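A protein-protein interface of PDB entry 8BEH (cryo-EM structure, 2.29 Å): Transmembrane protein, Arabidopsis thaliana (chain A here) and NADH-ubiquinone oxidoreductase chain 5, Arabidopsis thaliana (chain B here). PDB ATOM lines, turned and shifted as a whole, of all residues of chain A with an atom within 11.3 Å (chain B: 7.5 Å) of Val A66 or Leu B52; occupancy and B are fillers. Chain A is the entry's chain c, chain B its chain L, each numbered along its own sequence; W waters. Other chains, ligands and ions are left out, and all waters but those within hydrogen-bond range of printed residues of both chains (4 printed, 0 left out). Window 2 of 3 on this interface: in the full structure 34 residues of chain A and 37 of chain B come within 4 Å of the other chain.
The backbone carbonyl oxygen (O) of Gly B53 sits at hydrogen-bond distance from the backbone NH (N) of Val A66 (3.2 Å).
The side-chain carboxylate (OE1) of Glu B49 lies within salt-bridge range of the guanidinium group (NH1) of Arg A61 (3.2 Å).
The backbone carbonyl oxygen (O) of Ser B55 sits at hydrogen-bond distance from the guanidinium group (NH2) of Arg A61 (3.0 Å).
The backbone carbonyl oxygen (O) of His A63 lies within hydrogen-bond range of the side-chain hydroxyl (OG) of Ser B55, 2.7 Å away.
Of the 15 printed residues of chain B, 6 touch a printed residue of chain A.
Hydrophobic or aromatic side chains of chain B that line the printed part of chain A: Tyr B48.
Of the 13 printed residues of chain A, 7 touch a printed residue of chain B.
Printed residues of chain A that touch a printed residue of chain B: Arg A61, His A63, Pro A65, Val A66, Arg A67, Ile A69 and Pro A70.
Hydrophobic or aromatic side chains of chain A that line the printed part of chain B: His A63, Pro A65, Val A66, Ile A69 and Pro A70.
Among the printed residues, 11 pairs touch across the chains.
Among the printed residues, Asp or Glu carboxylates within 4 Å of a Lys or Arg side-chain nitrogen of the other chain: Arg A61 with Glu B49.
Printed residues of chain B within 4 Å of Val A66: Leu B52 and Gly B53.
Leu B52 touches two residues of chain A.
Tyr B48 touches just one residue of chain A: Arg A67 (3.2 Å).
No residue of chain A comes within 4 Å of Val B50.
No residue of chain A comes within 4 Å of Ala B51.
Gly B53 touches two residues of chain A.
Of the printed residues of chain B, Ile A69 touches Glu B49.
Printed residues of chain B within 4 Å of His A63: Ala B54 (3.98 Å) and Ser B55 (2.7 Å).
Printed residues of chain B within 4 Å of Pro A70: Glu B49 (3.3 Å).
Printed residues of chain A within 4 Å of Ala B54: His A63 (3.98 Å).
Printed residues of chain A within 4 Å of Glu B49: Arg A61, Ile A69 and Pro A70.
Phe B492 touches none of the printed residues of chain A.
The nearest printed residue of chain A that does not touch Leu B52 is Pro A65 (7.0 Å).
The nearest printed residue of chain B that does not touch Arg A61 is Val B50 (4.1 Å).
Water W2 bridges the side-chain hydroxyl of Tyr B48 (2.6 Å) and the backbone carbonyl oxygen of Pro A68 (2.8 Å).
Water W1 bridges the backbone NH of His A63 and the side-chain hydroxyl of Ser B55.
Water W3 lies within hydrogen-bond range of O of Tyr B48, NH1 of Arg A67 and N of Gly B53.
Water W4 bridges O of Leu B52 (2.8 Å) and NH1 of Arg A67 (2.9 Å).
O of Ala B54 touches CB of His A63 (3.98 Å).
Pro A65 touches Gly B53.
Leu B52 touches Val A66.
OH of Tyr B48 touches CD of Arg A67 (3.2 Å).
NH1 of Arg A67 touches O of Leu B52 (3.5 Å).
CB of Ile A69 touches CG of Glu B49, 3.4 Å away.
Glu B49 touches Pro A70.
The backbone carbonyl oxygen of Tyr B48 lies within hydrogen-bond range of the backbone NH of Gly B53, 3.0 Å away.
O of Arg A61 lies within hydrogen-bond range of N of Gly A79 (2.9 Å).
The backbone carbonyl oxygen (O) of Phe B47 is in hydrogen-bond range of the backbone NH (N) of Leu B52, 3.3 Å away.
O of Val B50 is in hydrogen-bond range of N of Ser B55 (3.2 Å).
N of Ile A69 is in hydrogen-bond range of OE1 of Gln A72 (3.1 Å).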
ATOM      1  N   ARG A  61      25.377 -15.967   4.665  1.00  0.00           N
ATOM      2  CA  ARG A  61      24.922 -16.232   3.301  1.00  0.00           C
ATOM      3  C   ARG A  61      25.695 -15.335   2.345  1.00  0.00           C
ATOM      4  O   ARG A  61      25.288 -14.193   2.084  1.00  0.00           O
ATOM      5  CB  ARG A  61      23.416 -16.014   3.171  1.00  0.00           C
ATOM      6  CG  ARG A  61      22.596 -16.489   4.362  1.00  0.00           C
ATOM      7  CD  ARG A  61      22.707 -17.996   4.559  1.00  0.00           C
ATOM      8  NE  ARG A  61      22.038 -18.743   3.502  1.00  0.00           N
ATOM      9  CZ  ARG A  61      20.731 -18.957   3.439  1.00  0.00           C
ATOM     10  NH1 ARG A  61      19.910 -18.500   4.366  1.00  0.00           N
ATOM     11  NH2 ARG A  61      20.238 -19.645   2.415  1.00  0.00           N
ATOM     12  N   PRO A  62      26.821 -15.805   1.807  1.00  0.00           N
ATOM     13  CA  PRO A  62      27.622 -14.947   0.921  1.00  0.00           C
ATOM     14  C   PRO A  62      26.921 -14.565  -0.372  1.00  0.00           C
ATOM     15  O   PRO A  62      27.299 -13.567  -0.994  1.00  0.00           O
ATOM     16  CB  PRO A  62      28.868 -15.799   0.643  1.00  0.00           C
ATOM     17  CG  PRO A  62      28.871 -16.853   1.697  1.00  0.00           C
ATOM     18  CD  PRO A  62      27.448 -17.120   2.014  1.00  0.00           C
ATOM     19  N   HIS A  63      25.921 -15.324  -0.803  1.00  0.00           N
ATOM     20  CA  HIS A  63      25.298 -15.127  -2.104  1.00  0.00           C
ATOM     21  C   HIS A  63      23.841 -14.733  -1.938  1.00  0.00           C
ATOM     22  O   HIS A  63      23.097 -15.383  -1.197  1.00  0.00           O
ATOM     23  CB  HIS A  63      25.400 -16.387  -2.957  1.00  0.00           C
ATOM     24  CG  HIS A  63      26.779 -16.648  -3.463  1.00  0.00           C
ATOM     25  ND1 HIS A  63      27.625 -15.634  -3.850  1.00  0.00           N
ATOM     26  CD2 HIS A  63      27.468 -17.800  -3.626  1.00  0.00           C
ATOM     27  CE1 HIS A  63      28.775 -16.151  -4.239  1.00  0.00           C
ATOM     28  NE2 HIS A  63      28.706 -17.463  -4.112  1.00  0.00           N
ATOM     29  N   MET A  64      23.445 -13.678  -2.630  1.00  0.00           N
ATOM     30  CA  MET A  64      22.040 -13.324  -2.704  1.00  0.00           C
ATOM     31  C   MET A  64      21.278 -14.439  -3.409  1.00  0.00           C
ATOM     32  O   MET A  64      21.744 -14.947  -4.437  1.00  0.00           O
ATOM     33  CB  MET A  64      21.858 -12.009  -3.456  1.00  0.00           C
ATOM     34  CG  MET A  64      22.406 -10.808  -2.733  1.00  0.00           C
ATOM     35  SD  MET A  64      21.889 -10.713  -1.010  1.00  0.00           S
ATOM     36  CE  MET A  64      20.227 -10.099  -1.215  1.00  0.00           C
ATOM     37  N   PRO A  65      20.132 -14.862  -2.887  1.00  0.00           N
ATOM     38  CA  PRO A  65      19.357 -15.904  -3.561  1.00  0.00           C
ATOM     39  C   PRO A  65      18.719 -15.380  -4.838  1.00  0.00           C
ATOM     40  O   PRO A  65      18.542 -14.176  -5.034  1.00  0.00           O
ATOM     41  CB  PRO A  65      18.300 -16.284  -2.521  1.00  0.00           C
ATOM     42  CG  PRO A  65      18.125 -15.046  -1.720  1.00  0.00           C
ATOM     43  CD  PRO A  65      19.485 -14.409  -1.644  1.00  0.00           C
ATOM     44  N   VAL A  66      18.378 -16.319  -5.722  1.00  0.00           N
ATOM     45  CA  VAL A  66      17.825 -15.947  -7.020  1.00  0.00           C
ATOM     46  C   VAL A  66      16.436 -15.339  -6.859  1.00  0.00           C
ATOM     47  O   VAL A  66      16.061 -14.416  -7.588  1.00  0.00           O
ATOM     48  CB  VAL A  66      17.817 -17.164  -7.963  1.00  0.00           C
ATOM     49  CG1 VAL A  66      19.232 -17.523  -8.356  1.00  0.00           C
ATOM     50  CG2 VAL A  66      17.120 -18.351  -7.322  1.00  0.00           C
ATOM     51  N   ARG A  67      15.658 -15.847  -5.918  1.00  0.00           N
ATOM     52  CA  ARG A  67      14.350 -15.324  -5.560  1.00  0.00           C
ATOM     53  C   ARG A  67      14.335 -15.098  -4.058  1.00  0.00           C
ATOM     54  O   ARG A  67      15.188 -15.630  -3.340  1.00  0.00           O
ATOM     55  CB  ARG A  67      13.221 -16.282  -5.968  1.00  0.00           C
ATOM     56  CG  ARG A  67      13.440 -17.723  -5.589  1.00  0.00           C
ATOM     57  CD  ARG A  67      12.283 -18.585  -6.052  1.00  0.00           C
ATOM     58  NE  ARG A  67      12.391 -18.947  -7.460  1.00  0.00           N
ATOM     59  CZ  ARG A  67      13.225 -19.856  -7.938  1.00  0.00           C
ATOM     60  NH1 ARG A  67      14.050 -20.521  -7.148  1.00  0.00           N
ATOM     61  NH2 ARG A  67      13.231 -20.108  -9.243  1.00  0.00           N
ATOM     62  N   PRO A  68      13.408 -14.284  -3.554  1.00  0.00           N
ATOM     63  CA  PRO A  68      13.356 -14.037  -2.106  1.00  0.00           C
ATOM     64  C   PRO A  68      13.108 -15.318  -1.319  1.00  0.00           C
ATOM     65  O   PRO A  68      12.352 -16.192  -1.743  1.00  0.00           O
ATOM     66  CB  PRO A  68      12.192 -13.050  -1.961  1.00  0.00           C
ATOM     67  CG  PRO A  68      11.396 -13.214  -3.208  1.00  0.00           C
ATOM     68  CD  PRO A  68      12.400 -13.484  -4.271  1.00  0.00           C
ATOM     69  N   ILE A  69      13.747 -15.415  -0.158  1.00  0.00           N
ATOM     70  CA  ILE A  69      13.683 -16.632   0.650  1.00  0.00           C
ATOM     71  C   ILE A  69      13.286 -16.264   2.074  1.00  0.00           C
ATOM     72  O   ILE A  69      13.469 -15.117   2.510  1.00  0.00           O
ATOM     73  CB  ILE A  69      15.025 -17.403   0.632  1.00  0.00           C
ATOM     74  CG1 ILE A  69      16.187 -16.501   1.049  1.00  0.00           C
ATOM     75  CG2 ILE A  69      15.260 -18.037  -0.723  1.00  0.00           C
ATOM     76  CD1 ILE A  69      17.466 -17.252   1.311  1.00  0.00           C
ATOM     77  N   PRO A  70      12.727 -17.221   2.824  1.00  0.00           N
ATOM     78  CA  PRO A  70      12.281 -16.916   4.195  1.00  0.00           C
ATOM     79  C   PRO A  70      13.379 -16.419   5.122  1.00  0.00           C
ATOM     80  O   PRO A  70      13.097 -15.614   6.015  1.00  0.00           O
ATOM     81  CB  PRO A  70      11.715 -18.258   4.680  1.00  0.00           C
ATOM     82  CG  PRO A  70      11.311 -18.957   3.451  1.00  0.00           C
ATOM     83  CD  PRO A  70      12.328 -18.578   2.415  1.00  0.00           C
ATOM     84  N   GLN A  72      15.611 -14.345   4.667  1.00  0.00           N
ATOM     85  CA  GLN A  72      15.816 -12.910   4.515  1.00  0.00           C
ATOM     86  C   GLN A  72      14.990 -12.092   5.495  1.00  0.00           C
ATOM     87  O   GLN A  72      15.297 -10.916   5.711  1.00  0.00           O
ATOM     88  CB  GLN A  72      15.493 -12.496   3.084  1.00  0.00           C
ATOM     89  CG  GLN A  72      16.623 -12.743   2.111  1.00  0.00           C
ATOM     90  CD  GLN A  72      16.209 -12.497   0.680  1.00  0.00           C
ATOM     91  OE1 GLN A  72      15.042 -12.639   0.335  1.00  0.00           O
ATOM     92  NE2 GLN A  72      17.162 -12.112  -0.155  1.00  0.00           N
ATOM     93  N   PHE A  78      23.476 -11.360   4.472  1.00  0.00           N
ATOM     94  CA  PHE A  78      23.466 -11.647   3.045  1.00  0.00           C
ATOM     95  C   PHE A  78      24.435 -10.716   2.327  1.00  0.00           C
ATOM     96  O   PHE A  78      24.345  -9.492   2.467  1.00  0.00           O
ATOM     97  CB  PHE A  78      22.058 -11.507   2.462  1.00  0.00           C
ATOM     98  CG  PHE A  78      21.163 -12.675   2.756  1.00  0.00           C
ATOM     99  CD1 PHE A  78      20.474 -12.757   3.956  1.00  0.00           C
ATOM    100  CD2 PHE A  78      21.029 -13.704   1.843  1.00  0.00           C
ATOM    101  CE1 PHE A  78      19.663 -13.838   4.230  1.00  0.00           C
ATOM    102  CE2 PHE A  78      20.222 -14.786   2.114  1.00  0.00           C
ATOM    103  CZ  PHE A  78      19.535 -14.853   3.307  1.00  0.00           C
ATOM    104  N   GLY A  79      25.353 -11.300   1.559  1.00  0.00           N
ATOM    105  CA  GLY A  79      26.326 -10.539   0.797  1.00  0.00           C
ATOM    106  C   GLY A  79      27.300  -9.730   1.630  1.00  0.00           C
ATOM    107  O   GLY A  79      27.540  -8.556   1.343  1.00  0.00           O
ATOM    108  N   LEU B  44      13.039 -29.220   4.075  1.00  0.00           N
ATOM    109  CA  LEU B  44      12.474 -28.869   2.774  1.00  0.00           C
ATOM    110  C   LEU B  44      12.649 -27.380   2.489  1.00  0.00           C
ATOM    111  O   LEU B  44      13.022 -26.987   1.374  1.00  0.00           O
ATOM    112  CB  LEU B  44      10.998 -29.254   2.721  1.00  0.00           C
ATOM    113  CG  LEU B  44      10.666 -30.730   2.486  1.00  0.00           C
ATOM    114  CD1 LEU B  44       9.169 -30.920   2.481  1.00  0.00           C
ATOM    115  CD2 LEU B  44      11.273 -31.228   1.187  1.00  0.00           C
ATOM    116  N   ALA B  46      14.978 -25.485   3.652  1.00  0.00           N
ATOM    117  CA  ALA B  46      16.399 -25.279   3.393  1.00  0.00           C
ATOM    118  C   ALA B  46      16.787 -25.752   1.996  1.00  0.00           C
ATOM    119  O   ALA B  46      17.672 -25.171   1.365  1.00  0.00           O
ATOM    120  CB  ALA B  46      17.240 -25.991   4.452  1.00  0.00           C
ATOM    121  N   PHE B  47      16.165 -26.827   1.513  1.00  0.00           N
ATOM    122  CA  PHE B  47      16.404 -27.256   0.140  1.00  0.00           C
ATOM    123  C   PHE B  47      15.942 -26.190  -0.841  1.00  0.00           C
ATOM    124  O   PHE B  47      16.614 -25.919  -1.840  1.00  0.00           O
ATOM    125  CB  PHE B  47      15.690 -28.576  -0.143  1.00  0.00           C
ATOM    126  CG  PHE B  47      15.891 -29.088  -1.544  1.00  0.00           C
ATOM    127  CD1 PHE B  47      15.017 -28.738  -2.561  1.00  0.00           C
ATOM    128  CD2 PHE B  47      16.951 -29.926  -1.841  1.00  0.00           C
ATOM    129  CE1 PHE B  47      15.206 -29.201  -3.849  1.00  0.00           C
ATOM    130  CE2 PHE B  47      17.141 -30.400  -3.127  1.00  0.00           C
ATOM    131  CZ  PHE B  47      16.265 -30.037  -4.132  1.00  0.00           C
ATOM    132  N   TYR B  48      14.790 -25.580  -0.564  1.00  0.00           N
ATOM    133  CA  TYR B  48      14.308 -24.495  -1.409  1.00  0.00           C
ATOM    134  C   TYR B  48      15.273 -23.312  -1.384  1.00  0.00           C
ATOM    135  O   TYR B  48      15.546 -22.699  -2.420  1.00  0.00           O
ATOM    136  CB  TYR B  48      12.909 -24.081  -0.954  1.00  0.00           C
ATOM    137  CG  TYR B  48      12.278 -22.932  -1.707  1.00  0.00           C
ATOM    138  CD1 TYR B  48      12.442 -21.623  -1.285  1.00  0.00           C
ATOM    139  CD2 TYR B  48      11.485 -23.168  -2.823  1.00  0.00           C
ATOM    140  CE1 TYR B  48      11.848 -20.576  -1.966  1.00  0.00           C
ATOM    141  CE2 TYR B  48      10.894 -22.133  -3.507  1.00  0.00           C
ATOM    142  CZ  TYR B  48      11.077 -20.840  -3.077  1.00  0.00           C
ATOM    143  OH  TYR B  48      10.480 -19.813  -3.763  1.00  0.00           O
ATOM    144  N   GLU B  49      15.811 -22.995  -0.206  1.00  0.00           N
ATOM    145  CA  GLU B  49      16.665 -21.822  -0.040  1.00  0.00           C
ATOM    146  C   GLU B  49      18.061 -22.017  -0.631  1.00  0.00           C
ATOM    147  O   GLU B  49      18.599 -21.106  -1.269  1.00  0.00           O
ATOM    148  CB  GLU B  49      16.776 -21.477   1.446  1.00  0.00           C
ATOM    149  CG  GLU B  49      15.736 -20.511   1.940  1.00  0.00           C
ATOM    150  CD  GLU B  49      16.026 -19.997   3.332  1.00  0.00           C
ATOM    151  OE1 GLU B  49      17.205 -19.992   3.736  1.00  0.00           O
ATOM    152  OE2 GLU B  49      15.073 -19.582   4.018  1.00  0.00           O
ATOM    153  N   VAL B  50      18.662 -23.182  -0.424  1.00  0.00           N
ATOM    154  CA  VAL B  50      20.079 -23.406  -0.698  1.00  0.00           C
ATOM    155  C   VAL B  50      20.304 -23.964  -2.094  1.00  0.00           C
ATOM    156  O   VAL B  50      21.148 -23.469  -2.838  1.00  0.00           O
ATOM    157  CB  VAL B  50      20.691 -24.336   0.377  1.00  0.00           C
ATOM    158  CG1 VAL B  50      22.086 -24.789  -0.029  1.00  0.00           C
ATOM    159  CG2 VAL B  50      20.717 -23.649   1.733  1.00  0.00           C
ATOM    160  N   ALA B  51      19.574 -25.016  -2.455  1.00  0.00           N
ATOM    161  CA  ALA B  51      19.785 -25.657  -3.745  1.00  0.00           C
ATOM    162  C   ALA B  51      19.027 -24.933  -4.854  1.00  0.00           C
ATOM    163  O   ALA B  51      19.616 -24.526  -5.858  1.00  0.00           O
ATOM    164  CB  ALA B  51      19.374 -27.129  -3.670  1.00  0.00           C
ATOM    165  N   LEU B  52      17.714 -24.766  -4.686  1.00  0.00           N
ATOM    166  CA  LEU B  52      16.924 -24.075  -5.702  1.00  0.00           C
ATOM    167  C   LEU B  52      17.238 -22.584  -5.731  1.00  0.00           C
ATOM    168  O   LEU B  52      17.240 -21.966  -6.800  1.00  0.00           O
ATOM    169  CB  LEU B  52      15.435 -24.311  -5.458  1.00  0.00           C
ATOM    170  CG  LEU B  52      15.004 -25.777  -5.353  1.00  0.00           C
ATOM    171  CD1 LEU B  52      13.517 -25.889  -5.102  1.00  0.00           C
ATOM    172  CD2 LEU B  52      15.399 -26.557  -6.595  1.00  0.00           C
ATOM    173  N   GLY B  53      17.504 -21.990  -4.569  1.00  0.00           N
ATOM    174  CA  GLY B  53      17.851 -20.585  -4.485  1.00  0.00           C
ATOM    175  C   GLY B  53      19.307 -20.257  -4.727  1.00  0.00           C
ATOM    176  O   GLY B  53      19.642 -19.077  -4.842  1.00  0.00           O
ATOM    177  N   ALA B  54      20.170 -21.271  -4.803  1.00  0.00           N
ATOM    178  CA  ALA B  54      21.607 -21.092  -5.022  1.00  0.00           C
ATOM    179  C   ALA B  54      22.214 -20.145  -3.988  1.00  0.00           C
ATOM    180  O   ALA B  54      22.939 -19.206  -4.316  1.00  0.00           O
ATOM    181  CB  ALA B  54      21.891 -20.610  -6.448  1.00  0.00           C
ATOM    182  N   SER B  55      21.909 -20.402  -2.716  1.00  0.00           N
ATOM    183  CA  SER B  55      22.391 -19.576  -1.604  1.00  0.00           C
ATOM    184  C   SER B  55      22.842 -20.505  -0.476  1.00  0.00           C
ATOM    185  O   SER B  55      22.052 -20.870   0.398  1.00  0.00           O
ATOM    186  CB  SER B  55      21.318 -18.603  -1.142  1.00  0.00           C
ATOM    187  OG  SER B  55      21.864 -17.598  -0.312  1.00  0.00           O
ATOM    188  N   SER B  80      24.417 -27.674  -1.758  1.00  0.00           N
ATOM    189  CA  SER B  80      23.430 -28.483  -2.472  1.00  0.00           C
ATOM    190  C   SER B  80      23.475 -29.944  -2.031  1.00  0.00           C
ATOM    191  O   SER B  80      22.437 -30.547  -1.732  1.00  0.00           O
ATOM    192  CB  SER B  80      23.653 -28.369  -3.981  1.00  0.00           C
ATOM    193  OG  SER B  80      23.302 -27.085  -4.455  1.00  0.00           O
ATOM    194  N   VAL B  83      21.887 -30.265   1.484  1.00  0.00           N
ATOM    195  CA  VAL B  83      20.432 -30.209   1.588  1.00  0.00           C
ATOM    196  C   VAL B  83      19.789 -31.424   0.929  1.00  0.00           C
ATOM    197  O   VAL B  83      18.717 -31.867   1.357  1.00  0.00           O
ATOM    198  CB  VAL B  83      19.876 -28.884   1.022  1.00  0.00           C
ATOM    199  CG1 VAL B  83      20.318 -27.717   1.888  1.00  0.00           C
ATOM    200  CG2 VAL B  83      20.274 -28.676  -0.428  1.00  0.00           C
ATOM    201  N   MET B 484      17.616 -31.765 -12.986  1.00  0.00           N
ATOM    202  CA  MET B 484      18.253 -31.034 -11.853  1.00  0.00           C
ATOM    203  C   MET B 484      19.592 -31.628 -11.439  1.00  0.00           C
ATOM    204  O   MET B 484      20.493 -30.915 -11.355  1.00  0.00           O
ATOM    205  CB  MET B 484      17.340 -31.034 -10.626  1.00  0.00           C
ATOM    206  CG  MET B 484      17.658 -30.064  -9.556  1.00  0.00           C
ATOM    207  SD  MET B 484      16.414 -30.175  -8.254  1.00  0.00           S
ATOM    208  CE  MET B 484      16.456 -31.929  -7.910  1.00  0.00           C
ATOM    209  N   PHE B 492      23.093 -27.200 -10.762  1.00  0.00           N
ATOM    210  CA  PHE B 492      22.357 -27.401  -9.517  1.00  0.00           C
ATOM    211  C   PHE B 492      23.302 -27.624  -8.339  1.00  0.00           C
ATOM    212  O   PHE B 492      23.039 -27.156  -7.229  1.00  0.00           O
ATOM    213  CB  PHE B 492      21.391 -28.574  -9.687  1.00  0.00           C
ATOM    214  CG  PHE B 492      20.915 -29.178  -8.396  1.00  0.00           C
ATOM    215  CD1 PHE B 492      19.870 -28.599  -7.692  1.00  0.00           C
ATOM    216  CD2 PHE B 492      21.494 -30.336  -7.897  1.00  0.00           C
ATOM    217  CE1 PHE B 492      19.418 -29.155  -6.514  1.00  0.00           C
ATOM    218  CE2 PHE B 492      21.051 -30.895  -6.712  1.00  0.00           C
ATOM    219  CZ  PHE B 492      20.010 -30.305  -6.020  1.00  0.00           C
HETATM  220  O   HOH W   1      25.007 -17.741   0.046  1.00  0.00           O
HETATM  221  O   HOH W   2      10.445 -17.244  -3.462  1.00  0.00           O
HETATM  222  O   HOH W   3      14.303 -20.833  -4.026  1.00  0.00           O
HETATM  223  O   HOH W   4      15.247 -22.789  -8.534  1.00  0.00           O
